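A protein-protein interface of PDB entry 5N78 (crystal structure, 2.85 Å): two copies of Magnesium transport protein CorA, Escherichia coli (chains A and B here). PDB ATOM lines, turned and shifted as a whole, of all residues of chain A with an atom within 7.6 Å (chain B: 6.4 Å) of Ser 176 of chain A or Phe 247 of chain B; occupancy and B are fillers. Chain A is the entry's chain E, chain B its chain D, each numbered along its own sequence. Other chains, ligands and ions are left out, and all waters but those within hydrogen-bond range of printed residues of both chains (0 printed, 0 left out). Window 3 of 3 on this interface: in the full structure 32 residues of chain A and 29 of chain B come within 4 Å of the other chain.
Among the printed residues, merely in contact across the chains: Ala 179 of chain A with Met 163 of chain B (3.3 Å), Met 245 of chain A with Gln 242 of chain B (3.4 Å), Ile 248 of chain A with Ile 250 of chain B (3.6 Å), Leu 175 of chain A with Phe 247 of chain B (3.6 Å), Asp 172 of chain A with Phe 247 of chain B (3.6 Å), Ile 248 of chain A with Asn 249 of chain B (3.7 Å), Leu 175 of chain A with Gly 246 of chain B (3.8 Å), Asp 172 of chain A with Ile 250 of chain B (3.9 Å), Met 245 of chain A with Gly 246 of chain B (3.9 Å), Met 241 of chain A with Gln 242 of chain B (3.9 Å), Leu 175 of chain A with Ala 243 of chain B (3.9 Å), Met 241 of chain A with Ala 243 of chain B (3.9 Å), Ser 176 of chain A with Phe 247 of chain B (3.95 Å) and Leu 175 of chain A with Ile 250 of chain B (3.98 Å).
NH1 of Arg 254 of chain B lies within salt-bridge range of OE1 of Glu 251 of chain B, 2.8 Å away.
OG of Ser 176 of chain A lies within hydrogen-bond range of O of Asp 172 of chain A.
Positions printed for both chains: 171, 245 and 248.
NH2 of Arg 254 of chain B is in salt-bridge range of OD2 of Asp 172 of chain A (2.8 Å).
Phe 247 of chain B touches three residues of chain A.
Gly 246 of chain B touches just these residues of chain A: Leu 175 (3.8 Å) and Met 245 (3.9 Å).
Of the printed residues of chain B, Met 245 of chain A touches Gln 242 (3.4 Å) and Gly 246 (3.9 Å).
Of the printed residues of chain A, Ala 243 of chain B touches Leu 175 (3.9 Å) and Met 241 (3.9 Å).
Of the printed residues of chain A, Met 163 of chain B touches Ala 179.
Of the printed residues of chain A, Arg 254 of chain B touches Asp 172.
Glu 164 of chain B touches none of the printed residues of chain A.
Glu 180 of chain A touches none of the printed residues of chain B.
The nearest residue of chain B that does not touch Ser 176 of chain A is Met 163 of chain B (4.3 Å).
Of the 17 printed residues of chain A, 7 touch a printed residue of chain B.
Hydrophobic or aromatic side chains of chain B that line the printed part of chain A: Met 163, Phe 247 and Ile 250.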
ATOM      1  N   LEU A 158      17.071 -12.105   5.599  1.00  0.00           N
ATOM      2  CA  LEU A 158      16.416 -11.169   6.462  1.00  0.00           C
ATOM      3  C   LEU A 158      15.638 -11.887   7.551  1.00  0.00           C
ATOM      4  O   LEU A 158      15.554 -11.417   8.679  1.00  0.00           O
ATOM      5  CB  LEU A 158      15.515 -10.305   5.622  1.00  0.00           C
ATOM      6  CG  LEU A 158      14.646  -9.319   6.365  1.00  0.00           C
ATOM      7  CD1 LEU A 158      15.495  -8.205   6.943  1.00  0.00           C
ATOM      8  CD2 LEU A 158      13.627  -8.748   5.405  1.00  0.00           C
ATOM      9  N   GLU A 170      20.222  -2.683  13.827  1.00  0.00           N
ATOM     10  CA  GLU A 170      19.873  -3.822  12.972  1.00  0.00           C
ATOM     11  C   GLU A 170      18.359  -3.929  12.634  1.00  0.00           C
ATOM     12  O   GLU A 170      17.998  -4.582  11.652  1.00  0.00           O
ATOM     13  CB  GLU A 170      20.373  -5.125  13.630  1.00  0.00           C
ATOM     14  N   TYR A 171      17.497  -3.283  13.428  1.00  0.00           N
ATOM     15  CA  TYR A 171      16.044  -3.403  13.277  1.00  0.00           C
ATOM     16  C   TYR A 171      15.366  -2.304  12.487  1.00  0.00           C
ATOM     17  O   TYR A 171      14.421  -2.577  11.773  1.00  0.00           O
ATOM     18  CB  TYR A 171      15.369  -3.567  14.632  1.00  0.00           C
ATOM     19  CG  TYR A 171      14.934  -4.999  14.851  1.00  0.00           C
ATOM     20  CD1 TYR A 171      15.849  -6.043  14.768  1.00  0.00           C
ATOM     21  CD2 TYR A 171      13.615  -5.312  15.117  1.00  0.00           C
ATOM     22  CE1 TYR A 171      15.454  -7.350  14.973  1.00  0.00           C
ATOM     23  CE2 TYR A 171      13.212  -6.615  15.317  1.00  0.00           C
ATOM     24  CZ  TYR A 171      14.132  -7.627  15.252  1.00  0.00           C
ATOM     25  OH  TYR A 171      13.711  -8.925  15.452  1.00  0.00           O
ATOM     26  N   ASP A 172      15.823  -1.064  12.602  1.00  0.00           N
ATOM     27  CA  ASP A 172      15.449  -0.056  11.609  1.00  0.00           C
ATOM     28  C   ASP A 172      15.724  -0.576  10.207  1.00  0.00           C
ATOM     29  O   ASP A 172      14.863  -0.497   9.321  1.00  0.00           O
ATOM     30  CB  ASP A 172      16.254   1.214  11.798  1.00  0.00           C
ATOM     31  CG  ASP A 172      15.503   2.261  12.553  1.00  0.00           C
ATOM     32  OD1 ASP A 172      14.342   2.520  12.167  1.00  0.00           O
ATOM     33  OD2 ASP A 172      16.078   2.832  13.518  1.00  0.00           O
ATOM     34  N   GLU A 173      16.921  -1.140  10.040  1.00  0.00           N
ATOM     35  CA  GLU A 173      17.407  -1.640   8.765  1.00  0.00           C
ATOM     36  C   GLU A 173      16.582  -2.834   8.274  1.00  0.00           C
ATOM     37  O   GLU A 173      16.400  -3.030   7.070  1.00  0.00           O
ATOM     38  CB  GLU A 173      18.873  -2.051   8.915  1.00  0.00           C
ATOM     39  CG  GLU A 173      19.651  -2.161   7.610  1.00  0.00           C
ATOM     40  CD  GLU A 173      20.181  -0.820   7.122  1.00  0.00           C
ATOM     41  OE1 GLU A 173      20.973  -0.173   7.849  1.00  0.00           O
ATOM     42  OE2 GLU A 173      19.824  -0.423   5.990  1.00  0.00           O
ATOM     43  N   ALA A 174      16.077  -3.628   9.211  1.00  0.00           N
ATOM     44  CA  ALA A 174      15.338  -4.812   8.860  1.00  0.00           C
ATOM     45  C   ALA A 174      13.950  -4.472   8.309  1.00  0.00           C
ATOM     46  O   ALA A 174      13.526  -5.063   7.316  1.00  0.00           O
ATOM     47  CB  ALA A 174      15.231  -5.740  10.063  1.00  0.00           C
ATOM     48  N   LEU A 175      13.229  -3.561   8.970  1.00  0.00           N
ATOM     49  CA  LEU A 175      11.925  -3.121   8.474  1.00  0.00           C
ATOM     50  C   LEU A 175      12.032  -2.431   7.140  1.00  0.00           C
ATOM     51  O   LEU A 175      11.190  -2.629   6.291  1.00  0.00           O
ATOM     52  CB  LEU A 175      11.273  -2.134   9.410  1.00  0.00           C
ATOM     53  CG  LEU A 175      10.794  -2.604  10.769  1.00  0.00           C
ATOM     54  CD1 LEU A 175       9.630  -1.709  11.182  1.00  0.00           C
ATOM     55  CD2 LEU A 175      10.384  -4.067  10.759  1.00  0.00           C
ATOM     56  N   SER A 176      13.059  -1.614   6.950  1.00  0.00           N
ATOM     57  CA  SER A 176      13.284  -1.010   5.645  1.00  0.00           C
ATOM     58  C   SER A 176      13.489  -2.030   4.564  1.00  0.00           C
ATOM     59  O   SER A 176      12.895  -1.914   3.498  1.00  0.00           O
ATOM     60  CB  SER A 176      14.494  -0.145   5.678  1.00  0.00           C
ATOM     61  OG  SER A 176      14.261   0.875   6.611  1.00  0.00           O
ATOM     62  N   THR A 177      14.290  -3.056   4.846  1.00  0.00           N
ATOM     63  CA  THR A 177      14.507  -4.115   3.870  1.00  0.00           C
ATOM     64  C   THR A 177      13.198  -4.823   3.566  1.00  0.00           C
ATOM     65  O   THR A 177      12.842  -4.984   2.415  1.00  0.00           O
ATOM     66  CB  THR A 177      15.546  -5.147   4.334  1.00  0.00           C
ATOM     67  OG1 THR A 177      16.732  -4.479   4.777  1.00  0.00           O
ATOM     68  CG2 THR A 177      15.923  -6.057   3.202  1.00  0.00           C
ATOM     69  N   LEU A 178      12.498  -5.275   4.593  1.00  0.00           N
ATOM     70  CA  LEU A 178      11.184  -5.856   4.402  1.00  0.00           C
ATOM     71  C   LEU A 178      10.294  -5.015   3.509  1.00  0.00           C
ATOM     72  O   LEU A 178       9.669  -5.530   2.599  1.00  0.00           O
ATOM     73  CB  LEU A 178      10.445  -5.957   5.711  1.00  0.00           C
ATOM     74  CG  LEU A 178      10.411  -7.273   6.416  1.00  0.00           C
ATOM     75  CD1 LEU A 178       9.372  -7.125   7.510  1.00  0.00           C
ATOM     76  CD2 LEU A 178      10.010  -8.394   5.484  1.00  0.00           C
ATOM     77  N   ALA A 179      10.199  -3.728   3.814  1.00  0.00           N
ATOM     78  CA  ALA A 179       9.380  -2.829   3.028  1.00  0.00           C
ATOM     79  C   ALA A 179       9.850  -2.709   1.573  1.00  0.00           C
ATOM     80  O   ALA A 179       9.042  -2.527   0.691  1.00  0.00           O
ATOM     81  CB  ALA A 179       9.373  -1.475   3.666  1.00  0.00           C
ATOM     82  N   GLU A 180      11.155  -2.799   1.325  1.00  0.00           N
ATOM     83  CA  GLU A 180      11.688  -2.764  -0.028  1.00  0.00           C
ATOM     84  C   GLU A 180      11.306  -4.063  -0.781  1.00  0.00           C
ATOM     85  O   GLU A 180      10.941  -4.044  -1.949  1.00  0.00           O
ATOM     86  CB  GLU A 180      13.195  -2.574   0.061  1.00  0.00           C
ATOM     87  CG  GLU A 180      13.930  -2.360  -1.276  1.00  0.00           C
ATOM     88  CD  GLU A 180      15.373  -2.931  -1.282  1.00  0.00           C
ATOM     89  OE1 GLU A 180      16.040  -2.942  -0.204  1.00  0.00           O
ATOM     90  OE2 GLU A 180      15.841  -3.395  -2.368  1.00  0.00           O
ATOM     91  N   LEU A 181      11.381  -5.198  -0.101  1.00  0.00           N
ATOM     92  CA  LEU A 181      11.010  -6.469  -0.698  1.00  0.00           C
ATOM     93  C   LEU A 181       9.497  -6.576  -0.980  1.00  0.00           C
ATOM     94  O   LEU A 181       9.091  -7.171  -1.971  1.00  0.00           O
ATOM     95  CB  LEU A 181      11.488  -7.643   0.179  1.00  0.00           C
ATOM     96  CG  LEU A 181      13.010  -7.752   0.293  1.00  0.00           C
ATOM     97  CD1 LEU A 181      13.470  -8.877   1.214  1.00  0.00           C
ATOM     98  CD2 LEU A 181      13.643  -7.938  -1.075  1.00  0.00           C
ATOM     99  N   GLU A 182       8.677  -6.012  -0.103  1.00  0.00           N
ATOM    100  CA  GLU A 182       7.247  -6.027  -0.324  1.00  0.00           C
ATOM    101  C   GLU A 182       6.998  -5.237  -1.588  1.00  0.00           C
ATOM    102  O   GLU A 182       6.281  -5.684  -2.474  1.00  0.00           O
ATOM    103  CB  GLU A 182       6.487  -5.407   0.841  1.00  0.00           C
ATOM    104  CG  GLU A 182       4.980  -5.605   0.806  1.00  0.00           C
ATOM    105  CD  GLU A 182       4.216  -4.512   0.054  1.00  0.00           C
ATOM    106  OE1 GLU A 182       4.840  -3.499  -0.348  1.00  0.00           O
ATOM    107  OE2 GLU A 182       2.974  -4.675  -0.166  1.00  0.00           O
ATOM    108  N   MET A 241       6.890  -9.015   9.516  1.00  0.00           N
ATOM    109  CA  MET A 241       6.548  -7.719  10.043  1.00  0.00           C
ATOM    110  C   MET A 241       5.958  -7.929  11.436  1.00  0.00           C
ATOM    111  O   MET A 241       6.411  -7.339  12.397  1.00  0.00           O
ATOM    112  CB  MET A 241       5.552  -7.066   9.078  1.00  0.00           C
ATOM    113  CG  MET A 241       5.056  -5.686   9.440  1.00  0.00           C
ATOM    114  SD  MET A 241       6.360  -4.471   9.577  1.00  0.00           S
ATOM    115  CE  MET A 241       6.850  -4.429   7.857  1.00  0.00           C
ATOM    116  N   MET A 245       7.640  -6.729  15.271  1.00  0.00           N
ATOM    117  CA  MET A 245       6.925  -5.933  16.249  1.00  0.00           C
ATOM    118  C   MET A 245       6.867  -6.676  17.553  1.00  0.00           C
ATOM    119  O   MET A 245       6.992  -6.072  18.624  1.00  0.00           O
ATOM    120  CB  MET A 245       5.525  -5.523  15.765  1.00  0.00           C
ATOM    121  CG  MET A 245       5.492  -4.057  15.330  1.00  0.00           C
ATOM    122  SD  MET A 245       4.124  -3.648  14.225  1.00  0.00           S
ATOM    123  CE  MET A 245       4.589  -4.439  12.694  1.00  0.00           C
ATOM    124  N   ILE A 248      10.367  -6.211  19.194  1.00  0.00           N
ATOM    125  CA  ILE A 248      10.414  -4.851  19.686  1.00  0.00           C
ATOM    126  C   ILE A 248       9.603  -4.643  20.965  1.00  0.00           C
ATOM    127  O   ILE A 248      10.038  -3.921  21.842  1.00  0.00           O
ATOM    128  CB  ILE A 248       9.883  -3.873  18.651  1.00  0.00           C
ATOM    129  CG1 ILE A 248      10.822  -3.797  17.466  1.00  0.00           C
ATOM    130  CG2 ILE A 248       9.781  -2.496  19.244  1.00  0.00           C
ATOM    131  CD1 ILE A 248      10.124  -3.312  16.208  1.00  0.00           C
ATOM    132  N   ILE B 162       7.687   6.988   4.528  1.00  0.00           N
ATOM    133  CA  ILE B 162       7.573   6.021   5.614  1.00  0.00           C
ATOM    134  C   ILE B 162       8.873   5.252   5.854  1.00  0.00           C
ATOM    135  O   ILE B 162       9.157   4.914   7.004  1.00  0.00           O
ATOM    136  CB  ILE B 162       6.344   5.103   5.422  1.00  0.00           C
ATOM    137  CG1 ILE B 162       5.081   5.901   5.760  1.00  0.00           C
ATOM    138  CG2 ILE B 162       6.395   3.881   6.332  1.00  0.00           C
ATOM    139  CD1 ILE B 162       3.785   5.265   5.315  1.00  0.00           C
ATOM    140  N   MET B 163       9.683   5.043   4.820  1.00  0.00           N
ATOM    141  CA  MET B 163      10.987   4.406   5.019  1.00  0.00           C
ATOM    142  C   MET B 163      12.063   5.339   5.562  1.00  0.00           C
ATOM    143  O   MET B 163      12.919   4.903   6.305  1.00  0.00           O
ATOM    144  CB  MET B 163      11.511   3.794   3.725  1.00  0.00           C
ATOM    145  CG  MET B 163      10.542   2.843   3.056  1.00  0.00           C
ATOM    146  SD  MET B 163       9.535   2.039   4.303  1.00  0.00           S
ATOM    147  CE  MET B 163       8.121   1.573   3.314  1.00  0.00           C
ATOM    148  N   GLU B 164      12.019   6.611   5.169  1.00  0.00           N
ATOM    149  CA  GLU B 164      13.135   7.548   5.366  1.00  0.00           C
ATOM    150  C   GLU B 164      12.995   8.435   6.619  1.00  0.00           C
ATOM    151  O   GLU B 164      13.991   8.742   7.254  1.00  0.00           O
ATOM    152  CB  GLU B 164      13.330   8.437   4.114  1.00  0.00           C
ATOM    153  N   GLY B 165      11.769   8.828   6.964  1.00  0.00           N
ATOM    154  CA  GLY B 165      11.508   9.763   8.076  1.00  0.00           C
ATOM    155  C   GLY B 165      11.521   9.150   9.476  1.00  0.00           C
ATOM    156  O   GLY B 165      11.057   8.016   9.653  1.00  0.00           O
ATOM    157  N   TYR B 171       5.252  11.928  10.621  1.00  0.00           N
ATOM    158  CA  TYR B 171       4.530  10.673  10.830  1.00  0.00           C
ATOM    159  C   TYR B 171       3.057  10.772  11.205  1.00  0.00           C
ATOM    160  O   TYR B 171       2.259   9.939  10.788  1.00  0.00           O
ATOM    161  CB  TYR B 171       5.264   9.819  11.847  1.00  0.00           C
ATOM    162  CG  TYR B 171       5.989   8.696  11.169  1.00  0.00           C
ATOM    163  CD1 TYR B 171       6.939   8.946  10.167  1.00  0.00           C
ATOM    164  CD2 TYR B 171       5.694   7.383  11.488  1.00  0.00           C
ATOM    165  CE1 TYR B 171       7.586   7.912   9.533  1.00  0.00           C
ATOM    166  CE2 TYR B 171       6.329   6.353  10.854  1.00  0.00           C
ATOM    167  CZ  TYR B 171       7.272   6.621   9.883  1.00  0.00           C
ATOM    168  OH  TYR B 171       7.886   5.570   9.266  1.00  0.00           O
ATOM    169  N   GLN B 242       1.058  -1.125   8.899  1.00  0.00           N
ATOM    170  CA  GLN B 242       1.852  -1.981   9.774  1.00  0.00           C
ATOM    171  C   GLN B 242       3.287  -1.514   9.932  1.00  0.00           C
ATOM    172  O   GLN B 242       3.838  -1.606  11.025  1.00  0.00           O
ATOM    173  CB  GLN B 242       1.820  -3.452   9.297  1.00  0.00           C
ATOM    174  CG  GLN B 242       0.557  -4.226   9.687  1.00  0.00           C
ATOM    175  CD  GLN B 242       0.104  -3.948  11.121  1.00  0.00           C
ATOM    176  OE1 GLN B 242       0.769  -4.352  12.092  1.00  0.00           O
ATOM    177  NE2 GLN B 242      -1.026  -3.240  11.260  1.00  0.00           N
ATOM    178  N   ALA B 243       3.916  -1.088   8.846  1.00  0.00           N
ATOM    179  CA  ALA B 243       5.330  -0.725   8.889  1.00  0.00           C
ATOM    180  C   ALA B 243       5.554   0.508   9.757  1.00  0.00           C
ATOM    181  O   ALA B 243       6.468   0.572  10.598  1.00  0.00           O
ATOM    182  CB  ALA B 243       5.830  -0.467   7.498  1.00  0.00           C
ATOM    183  N   ALA B 244       4.693   1.487   9.540  1.00  0.00           N
ATOM    184  CA  ALA B 244       4.712   2.713  10.309  1.00  0.00           C
ATOM    185  C   ALA B 244       4.620   2.450  11.804  1.00  0.00           C
ATOM    186  O   ALA B 244       5.432   2.953  12.583  1.00  0.00           O
ATOM    187  CB  ALA B 244       3.567   3.578   9.866  1.00  0.00           C
ATOM    188  N   MET B 245       3.673   1.622  12.207  1.00  0.00           N
ATOM    189  CA  MET B 245       3.585   1.254  13.606  1.00  0.00           C
ATOM    190  C   MET B 245       4.886   0.640  14.069  1.00  0.00           C
ATOM    191  O   MET B 245       5.331   0.883  15.179  1.00  0.00           O
ATOM    192  CB  MET B 245       2.394   0.342  13.904  1.00  0.00           C
ATOM    193  CG  MET B 245       1.243   1.111  14.569  1.00  0.00           C
ATOM    194  SD  MET B 245      -0.369   0.293  14.426  1.00  0.00           S
ATOM    195  CE  MET B 245      -0.760   0.536  12.701  1.00  0.00           C
ATOM    196  N   GLY B 246       5.521  -0.125  13.200  1.00  0.00           N
ATOM    197  CA  GLY B 246       6.822  -0.666  13.533  1.00  0.00           C
ATOM    198  C   GLY B 246       7.826   0.422  13.828  1.00  0.00           C
ATOM    199  O   GLY B 246       8.603   0.329  14.768  1.00  0.00           O
ATOM    200  N   PHE B 247       7.851   1.436  12.987  1.00  0.00           N
ATOM    201  CA  PHE B 247       8.830   2.488  13.146  1.00  0.00           C
ATOM    202  C   PHE B 247       8.568   3.337  14.394  1.00  0.00           C
ATOM    203  O   PHE B 247       9.507   3.732  15.097  1.00  0.00           O
ATOM    204  CB  PHE B 247       8.892   3.330  11.886  1.00  0.00           C
ATOM    205  CG  PHE B 247       9.604   2.658  10.767  1.00  0.00           C
ATOM    206  CD1 PHE B 247      10.946   2.353  10.886  1.00  0.00           C
ATOM    207  CD2 PHE B 247       8.929   2.327   9.579  1.00  0.00           C
ATOM    208  CE1 PHE B 247      11.605   1.737   9.856  1.00  0.00           C
ATOM    209  CE2 PHE B 247       9.589   1.692   8.530  1.00  0.00           C
ATOM    210  CZ  PHE B 247      10.934   1.403   8.678  1.00  0.00           C
ATOM    211  N   ILE B 248       7.293   3.593  14.654  1.00  0.00           N
ATOM    212  CA  ILE B 248       6.874   4.238  15.880  1.00  0.00           C
ATOM    213  C   ILE B 248       7.238   3.470  17.135  1.00  0.00           C
ATOM    214  O   ILE B 248       7.599   4.068  18.112  1.00  0.00           O
ATOM    215  CB  ILE B 248       5.362   4.438  15.898  1.00  0.00           C
ATOM    216  CG1 ILE B 248       4.968   5.463  14.850  1.00  0.00           C
ATOM    217  CG2 ILE B 248       4.893   4.928  17.264  1.00  0.00           C
ATOM    218  CD1 ILE B 248       3.529   5.308  14.435  1.00  0.00           C
ATOM    219  N   ASN B 249       7.124   2.151  17.119  1.00  0.00           N
ATOM    220  CA  ASN B 249       7.540   1.359  18.275  1.00  0.00           C
ATOM    221  C   ASN B 249       9.040   1.382  18.447  1.00  0.00           C
ATOM    222  O   ASN B 249       9.542   1.291  19.560  1.00  0.00           O
ATOM    223  CB  ASN B 249       7.129  -0.097  18.135  1.00  0.00           C
ATOM    224  CG  ASN B 249       5.687  -0.350  18.503  1.00  0.00           C
ATOM    225  OD1 ASN B 249       5.276  -1.513  18.571  1.00  0.00           O
ATOM    226  ND2 ASN B 249       4.899   0.711  18.716  1.00  0.00           N
ATOM    227  N   ILE B 250       9.760   1.433  17.331  1.00  0.00           N
ATOM    228  CA  ILE B 250      11.198   1.497  17.404  1.00  0.00           C
ATOM    229  C   ILE B 250      11.605   2.839  17.992  1.00  0.00           C
ATOM    230  O   ILE B 250      12.491   2.889  18.842  1.00  0.00           O
ATOM    231  CB  ILE B 250      11.850   1.286  16.032  1.00  0.00           C
ATOM    232  CG1 ILE B 250      11.874  -0.205  15.696  1.00  0.00           C
ATOM    233  CG2 ILE B 250      13.294   1.763  16.017  1.00  0.00           C
ATOM    234  CD1 ILE B 250      11.908  -0.477  14.209  1.00  0.00           C
ATOM    235  N   GLU B 251      10.964   3.903  17.523  1.00  0.00           N
ATOM    236  CA  GLU B 251      11.218   5.246  18.003  1.00  0.00           C
ATOM    237  C   GLU B 251      10.931   5.317  19.480  1.00  0.00           C
ATOM    238  O   GLU B 251      11.736   5.847  20.258  1.00  0.00           O
ATOM    239  CB  GLU B 251      10.337   6.246  17.263  1.00  0.00           C
ATOM    240  CG  GLU B 251      10.566   7.710  17.619  1.00  0.00           C
ATOM    241  CD  GLU B 251      12.027   8.136  17.484  1.00  0.00           C
ATOM    242  OE1 GLU B 251      12.779   7.517  16.687  1.00  0.00           O
ATOM    243  OE2 GLU B 251      12.432   9.112  18.157  1.00  0.00           O
ATOM    244  N   GLN B 252       9.797   4.767  19.880  1.00  0.00           N
ATOM    245  CA  GLN B 252       9.443   4.756  21.282  1.00  0.00           C
ATOM    246  C   GLN B 252      10.501   4.088  22.156  1.00  0.00           C
ATOM    247  O   GLN B 252      10.808   4.568  23.240  1.00  0.00           O
ATOM    248  CB  GLN B 252       8.126   4.067  21.486  1.00  0.00           C
ATOM    249  CG  GLN B 252       7.566   4.252  22.877  1.00  0.00           C
ATOM    250  CD  GLN B 252       6.194   3.647  22.992  1.00  0.00           C
ATOM    251  OE1 GLN B 252       6.035   2.568  23.537  1.00  0.00           O
ATOM    252  NE2 GLN B 252       5.196   4.322  22.430  1.00  0.00           N
ATOM    253  N   ARG B 254      13.633   4.055  21.504  1.00  0.00           N
ATOM    254  CA  ARG B 254      14.764   4.957  21.544  1.00  0.00           C
ATOM    255  C   ARG B 254      14.540   5.996  22.642  1.00  0.00           C
ATOM    256  O   ARG B 254      15.398   6.206  23.491  1.00  0.00           O
ATOM    257  CB  ARG B 254      14.950   5.656  20.202  1.00  0.00           C
ATOM    258  CG  ARG B 254      16.329   6.257  19.969  1.00  0.00           C
ATOM    259  CD  ARG B 254      16.591   6.541  18.500  1.00  0.00           C
ATOM    260  NE  ARG B 254      16.697   5.298  17.724  1.00  0.00           N
ATOM    261  CZ  ARG B 254      15.811   4.851  16.821  1.00  0.00           C
ATOM    262  NH1 ARG B 254      14.709   5.542  16.515  1.00  0.00           N
ATOM    263  NH2 ARG B 254      16.049   3.696  16.201  1.00  0.00           N
